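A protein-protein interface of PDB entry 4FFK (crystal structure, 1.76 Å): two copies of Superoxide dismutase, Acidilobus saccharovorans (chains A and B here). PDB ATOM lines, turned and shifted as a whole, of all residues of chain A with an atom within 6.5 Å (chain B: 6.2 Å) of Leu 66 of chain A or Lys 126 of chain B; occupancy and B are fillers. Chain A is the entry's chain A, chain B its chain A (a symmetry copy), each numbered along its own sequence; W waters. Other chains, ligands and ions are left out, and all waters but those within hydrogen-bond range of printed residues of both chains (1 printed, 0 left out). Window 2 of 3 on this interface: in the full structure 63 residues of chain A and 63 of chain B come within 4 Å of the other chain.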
ATOM      1  N   SER A  12       0.074  17.916   6.038  1.00  0.00           N
ATOM      2  CA  SER A  12       1.182  18.149   7.006  1.00  0.00           C
ATOM      3  C   SER A  12       2.399  17.291   6.624  1.00  0.00           C
ATOM      4  O   SER A  12       3.408  17.843   6.177  1.00  0.00           O
ATOM      5  CB  SER A  12       0.731  17.905   8.462  1.00  0.00           C
ATOM      6  N   VAL A  14       4.423  14.935   4.221  1.00  0.00           N
ATOM      7  CA  VAL A  14       4.456  14.536   2.821  1.00  0.00           C
ATOM      8  C   VAL A  14       4.873  13.067   2.676  1.00  0.00           C
ATOM      9  O   VAL A  14       5.899  12.640   3.199  1.00  0.00           O
ATOM     10  CB  VAL A  14       5.433  15.436   2.054  1.00  0.00           C
ATOM     11  CG1 VAL A  14       5.454  15.073   0.606  1.00  0.00           C
ATOM     12  CG2 VAL A  14       5.056  16.900   2.232  1.00  0.00           C
ATOM     13  N   LEU A  16       5.485  11.013  -0.697  1.00  0.00           N
ATOM     14  CA  LEU A  16       5.410  11.051  -2.151  1.00  0.00           C
ATOM     15  C   LEU A  16       5.276   9.633  -2.689  1.00  0.00           C
ATOM     16  O   LEU A  16       5.864   8.696  -2.118  1.00  0.00           O
ATOM     17  CB  LEU A  16       6.672  11.705  -2.679  1.00  0.00           C
ATOM     18  CG  LEU A  16       6.780  13.147  -2.195  1.00  0.00           C
ATOM     19  CD1 LEU A  16       8.000  13.781  -2.909  1.00  0.00           C
ATOM     20  CD2 LEU A  16       5.510  13.932  -2.485  1.00  0.00           C
ATOM     21  N   LYS A  61      14.756  12.892  -1.616  1.00  0.00           N
ATOM     22  CA  LYS A  61      15.361  14.159  -1.179  1.00  0.00           C
ATOM     23  C   LYS A  61      14.297  15.211  -0.947  1.00  0.00           C
ATOM     24  O   LYS A  61      14.359  15.939   0.042  1.00  0.00           O
ATOM     25  CB  LYS A  61      16.342  14.652  -2.248  1.00  0.00           C
ATOM     26  CG  LYS A  61      17.750  14.168  -2.071  1.00  0.00           C
ATOM     27  CD  LYS A  61      18.510  14.208  -3.413  1.00  0.00           C
ATOM     28  CE  LYS A  61      19.654  13.194  -3.403  1.00  0.00           C
ATOM     29  NZ  LYS A  61      19.877  12.406  -4.651  1.00  0.00           N
ATOM     30  N   LEU A  62      13.317  15.322  -1.860  1.00  0.00           N
ATOM     31  CA  LEU A  62      12.255  16.262  -1.754  1.00  0.00           C
ATOM     32  C   LEU A  62      11.427  16.070  -0.456  1.00  0.00           C
ATOM     33  O   LEU A  62      11.101  17.026   0.291  1.00  0.00           O
ATOM     34  CB  LEU A  62      11.308  15.979  -2.905  1.00  0.00           C
ATOM     35  CG  LEU A  62      10.847  16.993  -3.889  1.00  0.00           C
ATOM     36  CD1 LEU A  62      10.617  16.308  -5.249  1.00  0.00           C
ATOM     37  CD2 LEU A  62       9.576  17.518  -3.290  1.00  0.00           C
ATOM     38  N   GLU A  63      11.024  14.829  -0.271  1.00  0.00           N
ATOM     39  CA  GLU A  63      10.258  14.444   0.895  1.00  0.00           C
ATOM     40  C   GLU A  63      10.978  14.787   2.183  1.00  0.00           C
ATOM     41  O   GLU A  63      10.358  15.384   3.093  1.00  0.00           O
ATOM     42  CB  GLU A  63      10.021  12.939   0.837  1.00  0.00           C
ATOM     43  CG  GLU A  63       9.005  12.432   1.801  1.00  0.00           C
ATOM     44  CD  GLU A  63       8.638  11.025   1.369  1.00  0.00           C
ATOM     45  OE1 GLU A  63       9.465  10.127   1.619  1.00  0.00           O
ATOM     46  OE2 GLU A  63       7.618  10.868   0.695  1.00  0.00           O
ATOM     47  N   LYS A  64      12.250  14.429   2.264  1.00  0.00           N
ATOM     48  CA  LYS A  64      13.069  14.609   3.458  1.00  0.00           C
ATOM     49  C   LYS A  64      13.203  16.118   3.760  1.00  0.00           C
ATOM     50  O   LYS A  64      12.944  16.600   4.882  1.00  0.00           O
ATOM     51  CB  LYS A  64      14.451  13.993   3.266  1.00  0.00           C
ATOM     52  CG  LYS A  64      14.490  12.417   3.403  1.00  0.00           C
ATOM     53  CD  LYS A  64      15.886  11.938   3.654  1.00  0.00           C
ATOM     54  CE  LYS A  64      15.838  10.545   4.262  1.00  0.00           C
ATOM     55  NZ  LYS A  64      17.212   9.982   4.496  1.00  0.00           N
ATOM     56  N   TYR A  65      13.531  16.866   2.714  1.00  0.00           N
ATOM     57  CA  TYR A  65      13.455  18.308   2.812  1.00  0.00           C
ATOM     58  C   TYR A  65      12.104  18.831   3.313  1.00  0.00           C
ATOM     59  O   TYR A  65      12.083  19.625   4.250  1.00  0.00           O
ATOM     60  CB  TYR A  65      13.776  18.927   1.461  1.00  0.00           C
ATOM     61  CG  TYR A  65      13.479  20.393   1.435  1.00  0.00           C
ATOM     62  CD1 TYR A  65      12.328  20.875   0.806  1.00  0.00           C
ATOM     63  CD2 TYR A  65      14.358  21.303   2.035  1.00  0.00           C
ATOM     64  CE1 TYR A  65      12.055  22.240   0.777  1.00  0.00           C
ATOM     65  CE2 TYR A  65      14.081  22.675   2.006  1.00  0.00           C
ATOM     66  CZ  TYR A  65      12.926  23.124   1.377  1.00  0.00           C
ATOM     67  OH  TYR A  65      12.630  24.489   1.305  1.00  0.00           O
ATOM     68  N   LEU A  66      11.006  18.404   2.711  1.00  0.00           N
ATOM     69  CA  LEU A  66       9.665  18.936   3.011  1.00  0.00           C
ATOM     70  C   LEU A  66       9.139  18.524   4.380  1.00  0.00           C
ATOM     71  O   LEU A  66       8.334  19.263   4.994  1.00  0.00           O
ATOM     72  CB  LEU A  66       8.664  18.479   1.983  1.00  0.00           C
ATOM     73  CG  LEU A  66       8.792  19.179   0.629  1.00  0.00           C
ATOM     74  CD1 LEU A  66       8.034  18.345  -0.306  1.00  0.00           C
ATOM     75  CD2 LEU A  66       8.233  20.569   0.710  1.00  0.00           C
ATOM     76  N   ASN A  67       9.588  17.367   4.835  1.00  0.00           N
ATOM     77  CA  ASN A  67       9.204  16.870   6.155  1.00  0.00           C
ATOM     78  C   ASN A  67      10.241  17.250   7.202  1.00  0.00           C
ATOM     79  O   ASN A  67      10.158  16.826   8.355  1.00  0.00           O
ATOM     80  CB  ASN A  67       8.995  15.355   6.119  1.00  0.00           C
ATOM     81  CG  ASN A  67       7.763  14.955   5.328  1.00  0.00           C
ATOM     82  OD1 ASN A  67       6.771  15.681   5.246  1.00  0.00           O
ATOM     83  ND2 ASN A  67       7.821  13.775   4.747  1.00  0.00           N
ATOM     84  N   GLY A  68      11.230  18.035   6.798  1.00  0.00           N
ATOM     85  CA  GLY A  68      12.164  18.658   7.731  1.00  0.00           C
ATOM     86  C   GLY A  68      13.362  17.845   8.162  1.00  0.00           C
ATOM     87  O   GLY A  68      14.077  18.264   9.064  1.00  0.00           O
ATOM     88  N   GLN A  69      13.613  16.704   7.507  1.00  0.00           N
ATOM     89  CA  GLN A  69      14.795  15.887   7.784  1.00  0.00           C
ATOM     90  C   GLN A  69      16.071  16.398   7.113  1.00  0.00           C
ATOM     91  O   GLN A  69      17.167  16.215   7.630  1.00  0.00           O
ATOM     92  CB  GLN A  69      14.557  14.446   7.366  1.00  0.00           C
ATOM     93  CG  GLN A  69      13.275  13.828   7.903  1.00  0.00           C
ATOM     94  CD  GLN A  69      12.960  12.539   7.175  1.00  0.00           C
ATOM     95  OE1 GLN A  69      12.055  12.491   6.322  1.00  0.00           O
ATOM     96  NE2 GLN A  69      13.733  11.486   7.475  1.00  0.00           N
ATOM     97  N   LEU A  70      15.930  17.005   5.941  1.00  0.00           N
ATOM     98  CA  LEU A  70      16.945  17.772   5.250  1.00  0.00           C
ATOM     99  C   LEU A  70      16.600  19.222   5.411  1.00  0.00           C
ATOM    100  O   LEU A  70      15.486  19.681   5.158  1.00  0.00           O
ATOM    101  CB  LEU A  70      16.964  17.511   3.745  1.00  0.00           C
ATOM    102  CG  LEU A  70      17.220  16.135   3.137  1.00  0.00           C
ATOM    103  CD1 LEU A  70      17.303  16.298   1.566  1.00  0.00           C
ATOM    104  CD2 LEU A  70      18.472  15.442   3.719  1.00  0.00           C
ATOM    105  N   ILE A  73      17.766  21.921   0.413  1.00  0.00           N
ATOM    106  CA  ILE A  73      17.762  21.042  -0.753  1.00  0.00           C
ATOM    107  C   ILE A  73      18.249  21.913  -1.893  1.00  0.00           C
ATOM    108  O   ILE A  73      17.967  23.124  -1.939  1.00  0.00           O
ATOM    109  CB  ILE A  73      16.340  20.577  -1.046  1.00  0.00           C
ATOM    110  CG1 ILE A  73      16.319  19.505  -2.152  1.00  0.00           C
ATOM    111  CG2 ILE A  73      15.406  21.742  -1.406  1.00  0.00           C
ATOM    112  CD1 ILE A  73      14.932  18.943  -2.302  1.00  0.00           C
ATOM    113  N   PHE B 120       1.024  17.260  -0.988  1.00  0.00           N
ATOM    114  CA  PHE B 120       2.307  16.890  -1.598  1.00  0.00           C
ATOM    115  C   PHE B 120       3.485  17.757  -1.133  1.00  0.00           C
ATOM    116  O   PHE B 120       4.639  17.343  -1.223  1.00  0.00           O
ATOM    117  CB  PHE B 120       2.154  16.798  -3.116  1.00  0.00           C
ATOM    118  CG  PHE B 120       1.103  15.823  -3.539  1.00  0.00           C
ATOM    119  CD1 PHE B 120       1.206  14.465  -3.167  1.00  0.00           C
ATOM    120  CD2 PHE B 120       0.000  16.217  -4.297  1.00  0.00           C
ATOM    121  CE1 PHE B 120       0.236  13.548  -3.561  1.00  0.00           C
ATOM    122  CE2 PHE B 120      -1.008  15.290  -4.665  1.00  0.00           C
ATOM    123  CZ  PHE B 120      -0.885  13.961  -4.285  1.00  0.00           C
ATOM    124  N   PHE B 121       3.201  18.925  -0.556  1.00  0.00           N
ATOM    125  CA  PHE B 121       4.285  19.774  -0.046  1.00  0.00           C
ATOM    126  C   PHE B 121       4.148  20.137   1.433  1.00  0.00           C
ATOM    127  O   PHE B 121       5.010  20.826   2.004  1.00  0.00           O
ATOM    128  CB  PHE B 121       4.412  21.059  -0.871  1.00  0.00           C
ATOM    129  CG  PHE B 121       4.461  20.805  -2.339  1.00  0.00           C
ATOM    130  CD1 PHE B 121       3.279  20.690  -3.051  1.00  0.00           C
ATOM    131  CD2 PHE B 121       5.695  20.610  -2.978  1.00  0.00           C
ATOM    132  CE1 PHE B 121       3.273  20.435  -4.425  1.00  0.00           C
ATOM    133  CE2 PHE B 121       5.714  20.312  -4.364  1.00  0.00           C
ATOM    134  CZ  PHE B 121       4.506  20.258  -5.072  1.00  0.00           C
ATOM    135  N   GLY B 122       3.058  19.680   2.035  1.00  0.00           N
ATOM    136  CA  GLY B 122       2.915  19.845   3.482  1.00  0.00           C
ATOM    137  C   GLY B 122       2.025  21.021   3.804  1.00  0.00           C
ATOM    138  O   GLY B 122       1.114  20.911   4.650  1.00  0.00           O
ATOM    139  N   SER B 123       2.294  22.153   3.145  1.00  0.00           N
ATOM    140  CA  SER B 123       1.541  23.391   3.336  1.00  0.00           C
ATOM    141  C   SER B 123       1.727  24.233   2.116  1.00  0.00           C
ATOM    142  O   SER B 123       2.705  24.037   1.393  1.00  0.00           O
ATOM    143  CB  SER B 123       2.077  24.172   4.542  1.00  0.00           C
ATOM    144  OG  SER B 123       3.447  24.478   4.384  1.00  0.00           O
ATOM    145  N   PHE B 124       0.824  25.197   1.909  1.00  0.00           N
ATOM    146  CA  PHE B 124       1.047  26.185   0.879  1.00  0.00           C
ATOM    147  C   PHE B 124       2.374  26.930   1.022  1.00  0.00           C
ATOM    148  O   PHE B 124       3.056  27.207   0.014  1.00  0.00           O
ATOM    149  CB  PHE B 124      -0.092  27.171   0.746  1.00  0.00           C
ATOM    150  CG  PHE B 124       0.096  28.087  -0.412  1.00  0.00           C
ATOM    151  CD1 PHE B 124      -0.016  27.589  -1.717  1.00  0.00           C
ATOM    152  CD2 PHE B 124       0.461  29.418  -0.228  1.00  0.00           C
ATOM    153  CE1 PHE B 124       0.180  28.433  -2.821  1.00  0.00           C
ATOM    154  CE2 PHE B 124       0.667  30.258  -1.346  1.00  0.00           C
ATOM    155  CZ  PHE B 124       0.517  29.758  -2.630  1.00  0.00           C
ATOM    156  N   ASP B 125       2.754  27.259   2.256  1.00  0.00           N
ATOM    157  CA  ASP B 125       4.001  27.998   2.481  1.00  0.00           C
ATOM    158  C   ASP B 125       5.255  27.194   2.131  1.00  0.00           C
ATOM    159  O   ASP B 125       6.206  27.737   1.569  1.00  0.00           O
ATOM    160  CB  ASP B 125       4.061  28.573   3.923  1.00  0.00           C
ATOM    161  CG  ASP B 125       3.103  29.748   4.122  1.00  0.00           C
ATOM    162  OD1 ASP B 125       2.768  30.451   3.143  1.00  0.00           O
ATOM    163  OD2 ASP B 125       2.651  29.972   5.270  1.00  0.00           O
ATOM    164  N   LYS B 126       5.255  25.899   2.444  1.00  0.00           N
ATOM    165  CA  LYS B 126       6.365  25.038   2.078  1.00  0.00           C
ATOM    166  C   LYS B 126       6.422  24.886   0.543  1.00  0.00           C
ATOM    167  O   LYS B 126       7.496  24.954  -0.018  1.00  0.00           O
ATOM    168  CB  LYS B 126       6.294  23.681   2.757  1.00  0.00           C
ATOM    169  CG  LYS B 126       6.649  23.680   4.229  1.00  0.00           C
ATOM    170  CD  LYS B 126       6.123  22.394   4.864  1.00  0.00           C
ATOM    171  CE  LYS B 126       6.497  22.314   6.329  1.00  0.00           C
ATOM    172  NZ  LYS B 126       7.649  21.389   6.491  1.00  0.00           N
ATOM    173  N   PHE B 127       5.272  24.740  -0.091  1.00  0.00           N
ATOM    174  CA  PHE B 127       5.213  24.673  -1.552  1.00  0.00           C
ATOM    175  C   PHE B 127       5.710  25.992  -2.129  1.00  0.00           C
ATOM    176  O   PHE B 127       6.638  26.026  -2.948  1.00  0.00           O
ATOM    177  CB  PHE B 127       3.825  24.444  -2.033  1.00  0.00           C
ATOM    178  CG  PHE B 127       3.631  24.819  -3.480  1.00  0.00           C
ATOM    179  CD1 PHE B 127       4.202  24.037  -4.509  1.00  0.00           C
ATOM    180  CD2 PHE B 127       2.948  25.983  -3.822  1.00  0.00           C
ATOM    181  CE1 PHE B 127       4.008  24.411  -5.860  1.00  0.00           C
ATOM    182  CE2 PHE B 127       2.737  26.347  -5.143  1.00  0.00           C
ATOM    183  CZ  PHE B 127       3.302  25.550  -6.182  1.00  0.00           C
ATOM    184  N   LYS B 128       5.099  27.078  -1.685  1.00  0.00           N
ATOM    185  CA  LYS B 128       5.508  28.409  -2.148  1.00  0.00           C
ATOM    186  C   LYS B 128       7.019  28.648  -2.055  1.00  0.00           C
ATOM    187  O   LYS B 128       7.671  29.206  -2.987  1.00  0.00           O
ATOM    188  CB  LYS B 128       4.714  29.492  -1.416  1.00  0.00           C
ATOM    189  CG  LYS B 128       5.207  30.868  -1.762  1.00  0.00           C
ATOM    190  CD  LYS B 128       4.363  31.934  -1.096  1.00  0.00           C
ATOM    191  CE  LYS B 128       4.982  33.323  -1.332  1.00  0.00           C
ATOM    192  NZ  LYS B 128       3.910  34.353  -1.191  1.00  0.00           N
ATOM    193  N   LYS B 129       7.599  28.275  -0.929  1.00  0.00           N
ATOM    194  CA  LYS B 129       9.021  28.374  -0.769  1.00  0.00           C
ATOM    195  C   LYS B 129       9.796  27.516  -1.737  1.00  0.00           C
ATOM    196  O   LYS B 129      10.794  27.945  -2.287  1.00  0.00           O
ATOM    197  CB  LYS B 129       9.386  27.947   0.621  1.00  0.00           C
ATOM    198  CG  LYS B 129      10.860  27.722   0.890  1.00  0.00           C
ATOM    199  CD  LYS B 129      11.596  28.992   0.898  1.00  0.00           C
ATOM    200  CE  LYS B 129      13.064  28.708   1.197  1.00  0.00           C
ATOM    201  NZ  LYS B 129      13.913  29.666   0.404  1.00  0.00           N
ATOM    202  N   LEU B 130       9.369  26.282  -1.916  1.00  0.00           N
ATOM    203  CA  LEU B 130      10.162  25.404  -2.762  1.00  0.00           C
ATOM    204  C   LEU B 130       9.924  25.835  -4.206  1.00  0.00           C
ATOM    205  O   LEU B 130      10.849  25.872  -4.977  1.00  0.00           O
ATOM    206  CB  LEU B 130       9.718  23.971  -2.602  1.00  0.00           C
ATOM    207  CG  LEU B 130      10.402  22.849  -3.393  1.00  0.00           C
ATOM    208  CD1 LEU B 130      11.903  22.796  -3.115  1.00  0.00           C
ATOM    209  CD2 LEU B 130       9.705  21.495  -3.061  1.00  0.00           C
ATOM    210  N   PHE B 131       8.687  26.131  -4.545  1.00  0.00           N
ATOM    211  CA  PHE B 131       8.392  26.548  -5.914  1.00  0.00           C
ATOM    212  C   PHE B 131       9.115  27.846  -6.281  1.00  0.00           C
ATOM    213  O   PHE B 131       9.731  27.958  -7.364  1.00  0.00           O
ATOM    214  CB  PHE B 131       6.927  26.725  -6.110  1.00  0.00           C
ATOM    215  CG  PHE B 131       6.545  26.891  -7.560  1.00  0.00           C
ATOM    216  CD1 PHE B 131       6.347  28.131  -8.105  1.00  0.00           C
ATOM    217  CD2 PHE B 131       6.484  25.771  -8.401  1.00  0.00           C
ATOM    218  CE1 PHE B 131       5.985  28.253  -9.488  1.00  0.00           C
ATOM    219  CE2 PHE B 131       6.146  25.928  -9.771  1.00  0.00           C
ATOM    220  CZ  PHE B 131       5.881  27.156 -10.265  1.00  0.00           C
HETATM  221  O   HOH W   1       9.566  24.309   1.549  1.00  0.00           O
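No position is printed for both chains.
Of chain B, only Phe 120 (3.7 Å), Phe 121 (3.5 Å) and Lys 126 (2.7 Å) come within 4 Å of Leu 66 of chain A.
Of chain A, only Leu 66 comes within 4 Å of Lys 126 of chain B.
Of the printed residues of chain A, Lys 129 of chain B touches Tyr 65 (3.7 Å).
Of the printed residues of chain A, Leu 130 of chain B touches Leu 62 (3.99 Å) and Tyr 65 (3.9 Å).
The nearest residue of chain B that does not touch Leu 66 of chain A is Leu 130 of chain B (4.2 Å).
The nearest printed residue of chain B that does not touch Ser 12 of chain A is Phe 121 of chain B (5.3 Å).
Among the printed residues, merely in contact across the chains: Val 14 of chain A with Phe 120 of chain B (3.0 Å), Val 14 of chain A with Gly 122 of chain B (3.4 Å), Val 14 of chain A with Phe 121 of chain B (3.5 Å), Leu 66 of chain A with Phe 121 of chain B (3.5 Å), Leu 66 of chain A with Phe 120 of chain B (3.7 Å), Tyr 65 of chain A with Lys 129 of chain B (3.7 Å), Leu 16 of chain A with Phe 120 of chain B (3.7 Å), Tyr 65 of chain A with Leu 130 of chain B (3.9 Å) and Leu 62 of chain A with Leu 130 of chain B (3.99 Å).
Water W1 bridges O of Lys 126 of chain B (2.7 Å) and OH of Tyr 65 of chain A (3.1 Å).
The side-chain amide oxygen (OD1) of Asn 67 of chain A sits at hydrogen-bond distance from the backbone NH (N) of Val 14 of chain A (2.7 Å).
The backbone NH (N) of Leu 16 of chain A is in hydrogen-bond range of the side-chain carboxylate (OE2) of Glu 63 of chain A, at 2.6 Å.
The backbone NH (N) of Lys 126 of chain B sits at hydrogen-bond distance from the side-chain hydroxyl (OG) of Ser 123 of chain B, 3.0 Å away.
The backbone carbonyl oxygen (O) of Gly 122 of chain B lies within hydrogen-bond range of the backbone NH (N) of Ser 12 of chain A (3.5 Å).
The backbone carbonyl oxygen (O) of Leu 66 of chain A sits at hydrogen-bond distance from the side-chain amino group (NZ) of Lys 126 of chain B (2.7 Å).
Of the 12 printed residues of chain B, 6 touch a printed residue of chain A.
Along chain B the printed residues that touch a printed residue of chain A span positions 120 to 130.
Printed residues of chain A that touch a printed residue of chain B: Ser 12, Val 14, Leu 16, Leu 62, Tyr 65 and Leu 66.
Hydrophobic or aromatic side chains of chain A within 4 Å of the printed part of chain B: Val 14, Leu 16, Leu 62, Tyr 65 and Leu 66.
Along chain A the printed residues that touch a printed residue of chain B span positions 12 to 66.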
